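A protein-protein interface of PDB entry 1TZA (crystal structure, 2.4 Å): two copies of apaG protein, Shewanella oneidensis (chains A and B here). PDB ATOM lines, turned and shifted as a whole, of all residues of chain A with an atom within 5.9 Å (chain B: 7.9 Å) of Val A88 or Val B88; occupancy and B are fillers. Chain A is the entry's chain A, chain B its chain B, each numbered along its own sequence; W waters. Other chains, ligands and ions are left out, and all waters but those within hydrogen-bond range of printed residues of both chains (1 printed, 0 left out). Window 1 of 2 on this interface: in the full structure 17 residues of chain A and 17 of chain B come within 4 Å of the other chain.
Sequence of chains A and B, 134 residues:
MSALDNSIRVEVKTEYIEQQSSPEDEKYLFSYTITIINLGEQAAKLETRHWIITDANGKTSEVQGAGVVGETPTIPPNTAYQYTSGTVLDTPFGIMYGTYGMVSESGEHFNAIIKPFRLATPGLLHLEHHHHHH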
ATOM      1  N   GLN A  20     -19.295 -29.905   3.649  1.00  0.00           N
ATOM      2  CA  GLN A  20     -18.777 -29.181   4.806  1.00  0.00           C
ATOM      3  C   GLN A  20     -19.260 -27.741   4.769  1.00  0.00           C
ATOM      4  O   GLN A  20     -18.659 -26.864   5.388  1.00  0.00           O
ATOM      5  CB  GLN A  20     -17.246 -29.193   4.810  1.00  0.00           C
ATOM      6  CG  GLN A  20     -16.654 -30.577   4.731  1.00  0.00           C
ATOM      7  CD  GLN A  20     -17.200 -31.491   5.803  1.00  0.00           C
ATOM      8  OE1 GLN A  20     -17.234 -32.713   5.635  1.00  0.00           O
ATOM      9  NE2 GLN A  20     -17.631 -30.907   6.915  1.00  0.00           N
ATOM     10  N   GLU A  26     -20.281 -22.738   0.459  1.00  0.00           N
ATOM     11  CA  GLU A  26     -20.351 -24.122   0.022  1.00  0.00           C
ATOM     12  C   GLU A  26     -18.977 -24.767   0.095  1.00  0.00           C
ATOM     13  O   GLU A  26     -17.982 -24.175  -0.334  1.00  0.00           O
ATOM     14  CB  GLU A  26     -20.879 -24.203  -1.415  1.00  0.00           C
ATOM     15  CG  GLU A  26     -22.340 -23.816  -1.565  1.00  0.00           C
ATOM     16  CD  GLU A  26     -22.802 -23.806  -3.018  1.00  0.00           C
ATOM     17  OE1 GLU A  26     -22.489 -24.766  -3.761  1.00  0.00           O
ATOM     18  OE2 GLU A  26     -23.488 -22.838  -3.412  1.00  0.00           O
ATOM     19  N   LYS A  27     -18.930 -25.974   0.648  1.00  0.00           N
ATOM     20  CA  LYS A  27     -17.689 -26.734   0.765  1.00  0.00           C
ATOM     21  C   LYS A  27     -18.010 -28.205   0.543  1.00  0.00           C
ATOM     22  O   LYS A  27     -18.975 -28.730   1.098  1.00  0.00           O
ATOM     23  CB  LYS A  27     -17.062 -26.562   2.156  1.00  0.00           C
ATOM     24  CG  LYS A  27     -16.588 -25.159   2.491  1.00  0.00           C
ATOM     25  CD  LYS A  27     -16.195 -25.076   3.970  1.00  0.00           C
ATOM     26  CE  LYS A  27     -16.001 -23.634   4.438  1.00  0.00           C
ATOM     27  NZ  LYS A  27     -14.824 -22.968   3.806  1.00  0.00           N
ATOM     28  N   TYR A  28     -17.195 -28.869  -0.267  1.00  0.00           N
ATOM     29  CA  TYR A  28     -17.408 -30.277  -0.552  1.00  0.00           C
ATOM     30  C   TYR A  28     -16.104 -31.042  -0.370  1.00  0.00           C
ATOM     31  O   TYR A  28     -15.116 -30.766  -1.053  1.00  0.00           O
ATOM     32  CB  TYR A  28     -17.939 -30.441  -1.977  1.00  0.00           C
ATOM     33  CG  TYR A  28     -19.173 -29.618  -2.239  1.00  0.00           C
ATOM     34  CD1 TYR A  28     -19.077 -28.290  -2.658  1.00  0.00           C
ATOM     35  CD2 TYR A  28     -20.441 -30.152  -2.035  1.00  0.00           C
ATOM     36  CE1 TYR A  28     -20.222 -27.511  -2.866  1.00  0.00           C
ATOM     37  CE2 TYR A  28     -21.589 -29.386  -2.237  1.00  0.00           C
ATOM     38  CZ  TYR A  28     -21.471 -28.069  -2.652  1.00  0.00           C
ATOM     39  OH  TYR A  28     -22.602 -27.312  -2.837  1.00  0.00           O
ATOM     40  N   LEU A  29     -16.107 -31.994   0.565  1.00  0.00           N
ATOM     41  CA  LEU A  29     -14.923 -32.800   0.862  1.00  0.00           C
ATOM     42  C   LEU A  29     -14.813 -34.042  -0.024  1.00  0.00           C
ATOM     43  O   LEU A  29     -15.705 -34.890  -0.050  1.00  0.00           O
ATOM     44  CB  LEU A  29     -14.910 -33.226   2.339  1.00  0.00           C
ATOM     45  CG  LEU A  29     -13.794 -34.218   2.724  1.00  0.00           C
ATOM     46  CD1 LEU A  29     -12.421 -33.543   2.574  1.00  0.00           C
ATOM     47  CD2 LEU A  29     -13.980 -34.701   4.157  1.00  0.00           C
ATOM     48  N   PHE A  30     -13.699 -34.136  -0.738  1.00  0.00           N
ATOM     49  CA  PHE A  30     -13.430 -35.259  -1.627  1.00  0.00           C
ATOM     50  C   PHE A  30     -12.175 -35.993  -1.184  1.00  0.00           C
ATOM     51  O   PHE A  30     -11.285 -35.413  -0.575  1.00  0.00           O
ATOM     52  CB  PHE A  30     -13.184 -34.766  -3.058  1.00  0.00           C
ATOM     53  CG  PHE A  30     -14.427 -34.337  -3.785  1.00  0.00           C
ATOM     54  CD1 PHE A  30     -15.242 -35.283  -4.417  1.00  0.00           C
ATOM     55  CD2 PHE A  30     -14.767 -32.984  -3.874  1.00  0.00           C
ATOM     56  CE1 PHE A  30     -16.379 -34.885  -5.133  1.00  0.00           C
ATOM     57  CE2 PHE A  30     -15.899 -32.575  -4.585  1.00  0.00           C
ATOM     58  CZ  PHE A  30     -16.705 -33.529  -5.218  1.00  0.00           C
ATOM     59  N   GLY A  86      -7.018 -35.925   0.209  1.00  0.00           N
ATOM     60  CA  GLY A  86      -8.294 -35.332  -0.138  1.00  0.00           C
ATOM     61  C   GLY A  86      -8.219 -33.835  -0.353  1.00  0.00           C
ATOM     62  O   GLY A  86      -7.160 -33.224  -0.217  1.00  0.00           O
ATOM     63  N   THR A  87      -9.353 -33.238  -0.695  1.00  0.00           N
ATOM     64  CA  THR A  87      -9.395 -31.805  -0.908  1.00  0.00           C
ATOM     65  C   THR A  87     -10.823 -31.318  -0.761  1.00  0.00           C
ATOM     66  O   THR A  87     -11.765 -32.093  -0.935  1.00  0.00           O
ATOM     67  CB  THR A  87      -8.896 -31.431  -2.312  1.00  0.00           C
ATOM     68  OG1 THR A  87      -8.780 -30.008  -2.405  1.00  0.00           O
ATOM     69  CG2 THR A  87      -9.871 -31.918  -3.372  1.00  0.00           C
ATOM     70  N   VAL A  88     -10.975 -30.035  -0.438  1.00  0.00           N
ATOM     71  CA  VAL A  88     -12.291 -29.427  -0.269  1.00  0.00           C
ATOM     72  C   VAL A  88     -12.556 -28.421  -1.385  1.00  0.00           C
ATOM     73  O   VAL A  88     -11.784 -27.487  -1.566  1.00  0.00           O
ATOM     74  CB  VAL A  88     -12.396 -28.680   1.082  1.00  0.00           C
ATOM     75  CG1 VAL A  88     -13.710 -27.908   1.144  1.00  0.00           C
ATOM     76  CG2 VAL A  88     -12.320 -29.665   2.232  1.00  0.00           C
ATOM     77  N   LEU A  89     -13.641 -28.604  -2.133  1.00  0.00           N
ATOM     78  CA  LEU A  89     -13.964 -27.668  -3.212  1.00  0.00           C
ATOM     79  C   LEU A  89     -15.129 -26.774  -2.835  1.00  0.00           C
ATOM     80  O   LEU A  89     -15.963 -27.156  -2.018  1.00  0.00           O
ATOM     81  CB  LEU A  89     -14.342 -28.408  -4.492  1.00  0.00           C
ATOM     82  CG  LEU A  89     -13.269 -29.148  -5.278  1.00  0.00           C
ATOM     83  CD1 LEU A  89     -13.915 -29.719  -6.541  1.00  0.00           C
ATOM     84  CD2 LEU A  89     -12.124 -28.202  -5.635  1.00  0.00           C
ATOM     85  N   ASP A  90     -15.194 -25.590  -3.440  1.00  0.00           N
ATOM     86  CA  ASP A  90     -16.306 -24.686  -3.172  1.00  0.00           C
ATOM     87  C   ASP A  90     -17.456 -24.951  -4.145  1.00  0.00           C
ATOM     88  O   ASP A  90     -18.490 -24.288  -4.084  1.00  0.00           O
ATOM     89  CB  ASP A  90     -15.870 -23.208  -3.234  1.00  0.00           C
ATOM     90  CG  ASP A  90     -15.148 -22.856  -4.520  1.00  0.00           C
ATOM     91  OD1 ASP A  90     -15.323 -23.563  -5.538  1.00  0.00           O
ATOM     92  OD2 ASP A  90     -14.408 -21.852  -4.513  1.00  0.00           O
ATOM     93  N   GLU B  18      -2.531 -34.698   5.564  1.00  0.00           N
ATOM     94  CA  GLU B  18      -1.558 -34.037   4.704  1.00  0.00           C
ATOM     95  C   GLU B  18      -1.645 -32.503   4.726  1.00  0.00           C
ATOM     96  O   GLU B  18      -2.743 -31.937   4.804  1.00  0.00           O
ATOM     97  CB  GLU B  18      -1.769 -34.549   3.268  1.00  0.00           C
ATOM     98  CG  GLU B  18      -0.857 -33.940   2.224  1.00  0.00           C
ATOM     99  CD  GLU B  18      -1.174 -34.425   0.811  1.00  0.00           C
ATOM    100  OE1 GLU B  18      -2.256 -34.091   0.276  1.00  0.00           O
ATOM    101  OE2 GLU B  18      -0.332 -35.146   0.239  1.00  0.00           O
ATOM    102  N   GLN B  20      -1.586 -28.928   3.036  1.00  0.00           N
ATOM    103  CA  GLN B  20      -1.855 -28.355   1.720  1.00  0.00           C
ATOM    104  C   GLN B  20      -1.321 -26.931   1.580  1.00  0.00           C
ATOM    105  O   GLN B  20      -2.079 -25.968   1.680  1.00  0.00           O
ATOM    106  CB  GLN B  20      -3.358 -28.355   1.433  1.00  0.00           C
ATOM    107  CG  GLN B  20      -3.763 -29.318   0.330  1.00  0.00           C
ATOM    108  CD  GLN B  20      -4.291 -30.628   0.858  1.00  0.00           C
ATOM    109  OE1 GLN B  20      -5.459 -30.730   1.225  1.00  0.00           O
ATOM    110  NE2 GLN B  20      -3.432 -31.638   0.910  1.00  0.00           N
ATOM    111  N   GLU B  26      -1.281 -21.795   4.232  1.00  0.00           N
ATOM    112  CA  GLU B  26      -1.205 -23.207   4.591  1.00  0.00           C
ATOM    113  C   GLU B  26      -2.536 -23.749   5.116  1.00  0.00           C
ATOM    114  O   GLU B  26      -3.264 -23.061   5.828  1.00  0.00           O
ATOM    115  CB  GLU B  26      -0.101 -23.434   5.637  1.00  0.00           C
ATOM    116  CG  GLU B  26      -0.232 -22.590   6.904  1.00  0.00           C
ATOM    117  CD  GLU B  26       0.867 -22.877   7.926  1.00  0.00           C
ATOM    118  OE1 GLU B  26       2.062 -22.821   7.552  1.00  0.00           O
ATOM    119  OE2 GLU B  26       0.538 -23.152   9.103  1.00  0.00           O
ATOM    120  N   LYS B  27      -2.843 -24.988   4.740  1.00  0.00           N
ATOM    121  CA  LYS B  27      -4.072 -25.672   5.152  1.00  0.00           C
ATOM    122  C   LYS B  27      -3.672 -27.056   5.650  1.00  0.00           C
ATOM    123  O   LYS B  27      -2.634 -27.588   5.246  1.00  0.00           O
ATOM    124  CB  LYS B  27      -5.031 -25.837   3.971  1.00  0.00           C
ATOM    125  CG  LYS B  27      -5.506 -24.545   3.302  1.00  0.00           C
ATOM    126  CD  LYS B  27      -6.547 -23.778   4.116  1.00  0.00           C
ATOM    127  CE  LYS B  27      -7.098 -22.616   3.291  1.00  0.00           C
ATOM    128  NZ  LYS B  27      -8.070 -21.753   4.013  1.00  0.00           N
ATOM    129  N   TYR B  28      -4.483 -27.648   6.519  1.00  0.00           N
ATOM    130  CA  TYR B  28      -4.150 -28.967   7.034  1.00  0.00           C
ATOM    131  C   TYR B  28      -5.346 -29.903   7.013  1.00  0.00           C
ATOM    132  O   TYR B  28      -6.373 -29.622   7.624  1.00  0.00           O
ATOM    133  CB  TYR B  28      -3.588 -28.852   8.452  1.00  0.00           C
ATOM    134  CG  TYR B  28      -2.343 -28.000   8.531  1.00  0.00           C
ATOM    135  CD1 TYR B  28      -2.420 -26.601   8.546  1.00  0.00           C
ATOM    136  CD2 TYR B  28      -1.082 -28.588   8.584  1.00  0.00           C
ATOM    137  CE1 TYR B  28      -1.264 -25.812   8.619  1.00  0.00           C
ATOM    138  CE2 TYR B  28       0.077 -27.813   8.652  1.00  0.00           C
ATOM    139  CZ  TYR B  28      -0.022 -26.429   8.671  1.00  0.00           C
ATOM    140  OH  TYR B  28       1.123 -25.672   8.751  1.00  0.00           O
ATOM    141  N   LEU B  29      -5.205 -31.018   6.300  1.00  0.00           N
ATOM    142  CA  LEU B  29      -6.287 -31.998   6.179  1.00  0.00           C
ATOM    143  C   LEU B  29      -6.214 -33.084   7.244  1.00  0.00           C
ATOM    144  O   LEU B  29      -5.188 -33.749   7.403  1.00  0.00           O
ATOM    145  CB  LEU B  29      -6.265 -32.657   4.791  1.00  0.00           C
ATOM    146  CG  LEU B  29      -7.217 -33.842   4.562  1.00  0.00           C
ATOM    147  CD1 LEU B  29      -8.674 -33.383   4.693  1.00  0.00           C
ATOM    148  CD2 LEU B  29      -6.973 -34.449   3.176  1.00  0.00           C
ATOM    149  N   PHE B  30      -7.319 -33.260   7.961  1.00  0.00           N
ATOM    150  CA  PHE B  30      -7.421 -34.277   9.001  1.00  0.00           C
ATOM    151  C   PHE B  30      -8.569 -35.204   8.645  1.00  0.00           C
ATOM    152  O   PHE B  30      -9.495 -34.802   7.932  1.00  0.00           O
ATOM    153  CB  PHE B  30      -7.734 -33.634  10.353  1.00  0.00           C
ATOM    154  CG  PHE B  30      -6.610 -32.843  10.923  1.00  0.00           C
ATOM    155  CD1 PHE B  30      -5.642 -33.460  11.719  1.00  0.00           C
ATOM    156  CD2 PHE B  30      -6.507 -31.475  10.672  1.00  0.00           C
ATOM    157  CE1 PHE B  30      -4.580 -32.723  12.268  1.00  0.00           C
ATOM    158  CE2 PHE B  30      -5.450 -30.728  11.211  1.00  0.00           C
ATOM    159  CZ  PHE B  30      -4.487 -31.360  12.013  1.00  0.00           C
ATOM    160  N   SER B  31      -8.511 -36.436   9.140  1.00  0.00           N
ATOM    161  CA  SER B  31      -9.587 -37.394   8.922  1.00  0.00           C
ATOM    162  C   SER B  31     -10.034 -37.785  10.321  1.00  0.00           C
ATOM    163  O   SER B  31      -9.250 -37.715  11.264  1.00  0.00           O
ATOM    164  CB  SER B  31      -9.087 -38.641   8.200  1.00  0.00           C
ATOM    165  OG  SER B  31      -8.447 -39.526   9.104  1.00  0.00           O
ATOM    166  N   TYR B  32     -11.294 -38.164  10.466  1.00  0.00           N
ATOM    167  CA  TYR B  32     -11.795 -38.588  11.755  1.00  0.00           C
ATOM    168  C   TYR B  32     -12.749 -39.741  11.542  1.00  0.00           C
ATOM    169  O   TYR B  32     -13.591 -39.712  10.647  1.00  0.00           O
ATOM    170  CB  TYR B  32     -12.460 -37.425  12.512  1.00  0.00           C
ATOM    171  CG  TYR B  32     -13.609 -36.736  11.817  1.00  0.00           C
ATOM    172  CD1 TYR B  32     -14.873 -37.317  11.782  1.00  0.00           C
ATOM    173  CD2 TYR B  32     -13.436 -35.483  11.213  1.00  0.00           C
ATOM    174  CE1 TYR B  32     -15.944 -36.673  11.164  1.00  0.00           C
ATOM    175  CE2 TYR B  32     -14.495 -34.830  10.596  1.00  0.00           C
ATOM    176  CZ  TYR B  32     -15.752 -35.433  10.574  1.00  0.00           C
ATOM    177  OH  TYR B  32     -16.820 -34.805   9.979  1.00  0.00           O
ATOM    178  N   ILE B  53     -16.097 -26.409  14.775  1.00  0.00           N
ATOM    179  CA  ILE B  53     -14.665 -26.577  14.641  1.00  0.00           C
ATOM    180  C   ILE B  53     -13.940 -25.299  15.000  1.00  0.00           C
ATOM    181  O   ILE B  53     -14.349 -24.210  14.599  1.00  0.00           O
ATOM    182  CB  ILE B  53     -14.346 -27.013  13.196  1.00  0.00           C
ATOM    183  CG1 ILE B  53     -15.088 -28.327  12.915  1.00  0.00           C
ATOM    184  CG2 ILE B  53     -12.847 -27.175  12.989  1.00  0.00           C
ATOM    185  CD1 ILE B  53     -15.267 -28.652  11.418  1.00  0.00           C
ATOM    186  N   ASP B  55      -9.909 -23.655  15.276  1.00  0.00           N
ATOM    187  CA  ASP B  55      -8.482 -23.813  15.028  1.00  0.00           C
ATOM    188  C   ASP B  55      -7.622 -23.104  16.071  1.00  0.00           C
ATOM    189  O   ASP B  55      -8.139 -22.419  16.952  1.00  0.00           O
ATOM    190  CB  ASP B  55      -8.109 -23.321  13.621  1.00  0.00           C
ATOM    191  CG  ASP B  55      -8.519 -21.875  13.359  1.00  0.00           C
ATOM    192  OD1 ASP B  55      -8.243 -20.983  14.198  1.00  0.00           O
ATOM    193  OD2 ASP B  55      -9.110 -21.623  12.286  1.00  0.00           O
ATOM    194  N   SER B  61     -15.774 -22.386  12.814  1.00  0.00           N
ATOM    195  CA  SER B  61     -16.713 -22.652  11.726  1.00  0.00           C
ATOM    196  C   SER B  61     -17.702 -23.746  12.156  1.00  0.00           C
ATOM    197  O   SER B  61     -17.405 -24.554  13.038  1.00  0.00           O
ATOM    198  CB  SER B  61     -15.973 -23.085  10.450  1.00  0.00           C
ATOM    199  OG  SER B  61     -15.407 -24.379  10.571  1.00  0.00           O
ATOM    200  N   GLY B  86     -13.611 -35.923   7.338  1.00  0.00           N
ATOM    201  CA  GLY B  86     -12.440 -35.108   7.579  1.00  0.00           C
ATOM    202  C   GLY B  86     -12.764 -33.637   7.581  1.00  0.00           C
ATOM    203  O   GLY B  86     -13.907 -33.243   7.389  1.00  0.00           O
ATOM    204  N   THR B  87     -11.749 -32.822   7.816  1.00  0.00           N
ATOM    205  CA  THR B  87     -11.918 -31.380   7.820  1.00  0.00           C
ATOM    206  C   THR B  87     -10.573 -30.775   7.487  1.00  0.00           C
ATOM    207  O   THR B  87      -9.529 -31.380   7.744  1.00  0.00           O
ATOM    208  CB  THR B  87     -12.365 -30.840   9.198  1.00  0.00           C
ATOM    209  OG1 THR B  87     -12.927 -29.532   9.032  1.00  0.00           O
ATOM    210  CG2 THR B  87     -11.171 -30.735  10.145  1.00  0.00           C
ATOM    211  N   VAL B  88     -10.602 -29.589   6.900  1.00  0.00           N
ATOM    212  CA  VAL B  88      -9.377 -28.896   6.554  1.00  0.00           C
ATOM    213  C   VAL B  88      -9.273 -27.705   7.479  1.00  0.00           C
ATOM    214  O   VAL B  88     -10.189 -26.882   7.537  1.00  0.00           O
ATOM    215  CB  VAL B  88      -9.400 -28.389   5.101  1.00  0.00           C
ATOM    216  CG1 VAL B  88      -8.141 -27.548   4.827  1.00  0.00           C
ATOM    217  CG2 VAL B  88      -9.496 -29.572   4.142  1.00  0.00           C
ATOM    218  N   LEU B  89      -8.167 -27.626   8.210  1.00  0.00           N
ATOM    219  CA  LEU B  89      -7.938 -26.525   9.140  1.00  0.00           C
ATOM    220  C   LEU B  89      -6.932 -25.554   8.561  1.00  0.00           C
ATOM    221  O   LEU B  89      -6.188 -25.890   7.641  1.00  0.00           O
ATOM    222  CB  LEU B  89      -7.389 -27.034  10.481  1.00  0.00           C
ATOM    223  CG  LEU B  89      -8.267 -27.789  11.486  1.00  0.00           C
ATOM    224  CD1 LEU B  89      -7.500 -27.891  12.789  1.00  0.00           C
ATOM    225  CD2 LEU B  89      -9.578 -27.062  11.724  1.00  0.00           C
ATOM    226  N   ASP B  90      -6.914 -24.345   9.108  1.00  0.00           N
ATOM    227  CA  ASP B  90      -5.964 -23.336   8.665  1.00  0.00           C
ATOM    228  C   ASP B  90      -4.723 -23.458   9.538  1.00  0.00           C
ATOM    229  O   ASP B  90      -3.681 -22.881   9.229  1.00  0.00           O
ATOM    230  CB  ASP B  90      -6.563 -21.930   8.808  1.00  0.00           C
ATOM    231  CG  ASP B  90      -7.688 -21.666   7.813  1.00  0.00           C
ATOM    232  OD1 ASP B  90      -8.381 -20.629   7.949  1.00  0.00           O
ATOM    233  OD2 ASP B  90      -7.877 -22.489   6.890  1.00  0.00           O
ATOM    234  N   THR B  91      -4.840 -24.216  10.628  1.00  0.00           N
ATOM    235  CA  THR B  91      -3.726 -24.404  11.557  1.00  0.00           C
ATOM    236  C   THR B  91      -3.421 -25.878  11.770  1.00  0.00           C
ATOM    237  O   THR B  91      -4.265 -26.735  11.525  1.00  0.00           O
ATOM    238  CB  THR B  91      -4.024 -23.759  12.926  1.00  0.00           C
ATOM    239  OG1 THR B  91      -5.149 -24.410  13.529  1.00  0.00           O
ATOM    240  CG2 THR B  91      -4.339 -22.279  12.746  1.00  0.00           C
ATOM    241  N   MET B  96     -12.503 -29.955  18.093  1.00  0.00           N
ATOM    242  CA  MET B  96     -13.747 -30.231  17.399  1.00  0.00           C
ATOM    243  C   MET B  96     -14.726 -30.941  18.335  1.00  0.00           C
ATOM    244  O   MET B  96     -14.345 -31.848  19.071  1.00  0.00           O
ATOM    245  CB  MET B  96     -13.432 -31.098  16.176  1.00  0.00           C
ATOM    246  CG  MET B  96     -14.553 -31.256  15.164  1.00  0.00           C
ATOM    247  SD  MET B  96     -13.900 -31.989  13.455  1.00  0.00           S
ATOM    248  CE  MET B  96     -15.582 -31.970  12.508  1.00  0.00           C
ATOM    249  N   LEU B 119      -7.489 -32.256  17.109  1.00  0.00           N
ATOM    250  CA  LEU B 119      -7.044 -32.388  15.730  1.00  0.00           C
ATOM    251  C   LEU B 119      -5.619 -31.837  15.811  1.00  0.00           C
ATOM    252  O   LEU B 119      -5.427 -30.680  16.189  1.00  0.00           O
ATOM    253  CB  LEU B 119      -7.892 -31.527  14.787  1.00  0.00           C
ATOM    254  CG  LEU B 119      -9.274 -32.054  14.383  1.00  0.00           C
ATOM    255  CD1 LEU B 119      -9.910 -31.094  13.384  1.00  0.00           C
ATOM    256  CD2 LEU B 119      -9.137 -33.439  13.770  1.00  0.00           C
HETATM  257  O   HOH W   1     -15.235 -29.139   7.809  1.00  0.00           O
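Of the printed residues of chain B, Leu A29 touches Gly B86.
Printed residues of chain B within 4 Å of Gly A86: Gln B20 and Leu B29.
Val A88 touches just one residue of chain B: Val B88 (3.4 Å).
Val B88 touches one residue of chain A.
The nearest residue of chain A that does not touch Val B88 is Leu A29 (5.2 Å).
The nearest printed residue of chain B that does not touch Gly A86 is Glu B18 (5.0 Å).
Gln A20 touches Gly B86, and with the chains exchanged Gly A86 touches Gln B20.
Leu A29 touches Gly B86, and with the chains exchanged Gly A86 touches Leu B29.
Val B88 touches its own counterpart, Val A88.
Positions printed for both chains: 20, 26, 27, 28, 29, 30, 86, 87, 88, 89 and 90.
Of the 5 pairs that touch across the chains among the printed residues, 5 have their exchanged pair printed and touching as well.
Printed residues of chain B that touch a printed residue of chain A: Gln B20, Leu B29, Gly B86 and Val B88.
Hydrophobic or aromatic side chains of chain B within 4 Å of the printed part of chain A: Leu B29 and Val B88.
Among the printed residues, no Asp or Glu carboxylate lies within 4 Å of a Lys or Arg side-chain nitrogen of the other chain.
O of Gly A86 sits close to OE1 of Gln B20.
Among the printed residues, merely in contact across the chains: Gln A20 with Gly B86, Leu A29 with Gly B86, Gly A86 with Leu B29 and Val A88 with Val B88.
Water W1 lies within hydrogen-bond range of the side-chain hydroxyl of Thr B87 (2.6 Å) and the side-chain amide nitrogen of Gln A20 (3.1 Å).
N of Gln A20 is in hydrogen-bond range of O of Lys A27.
The backbone carbonyl oxygen (O) of Lys B27 lies within hydrogen-bond range of the backbone NH (N) of Gln B20, at 2.8 Å.
O of Glu B18 lies within hydrogen-bond range of N of Leu B29 (3.0 Å).
The side-chain carboxylate of Glu B18 lies within hydrogen-bond range of the side-chain amide nitrogen of Gln B20, at 2.8 Å.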
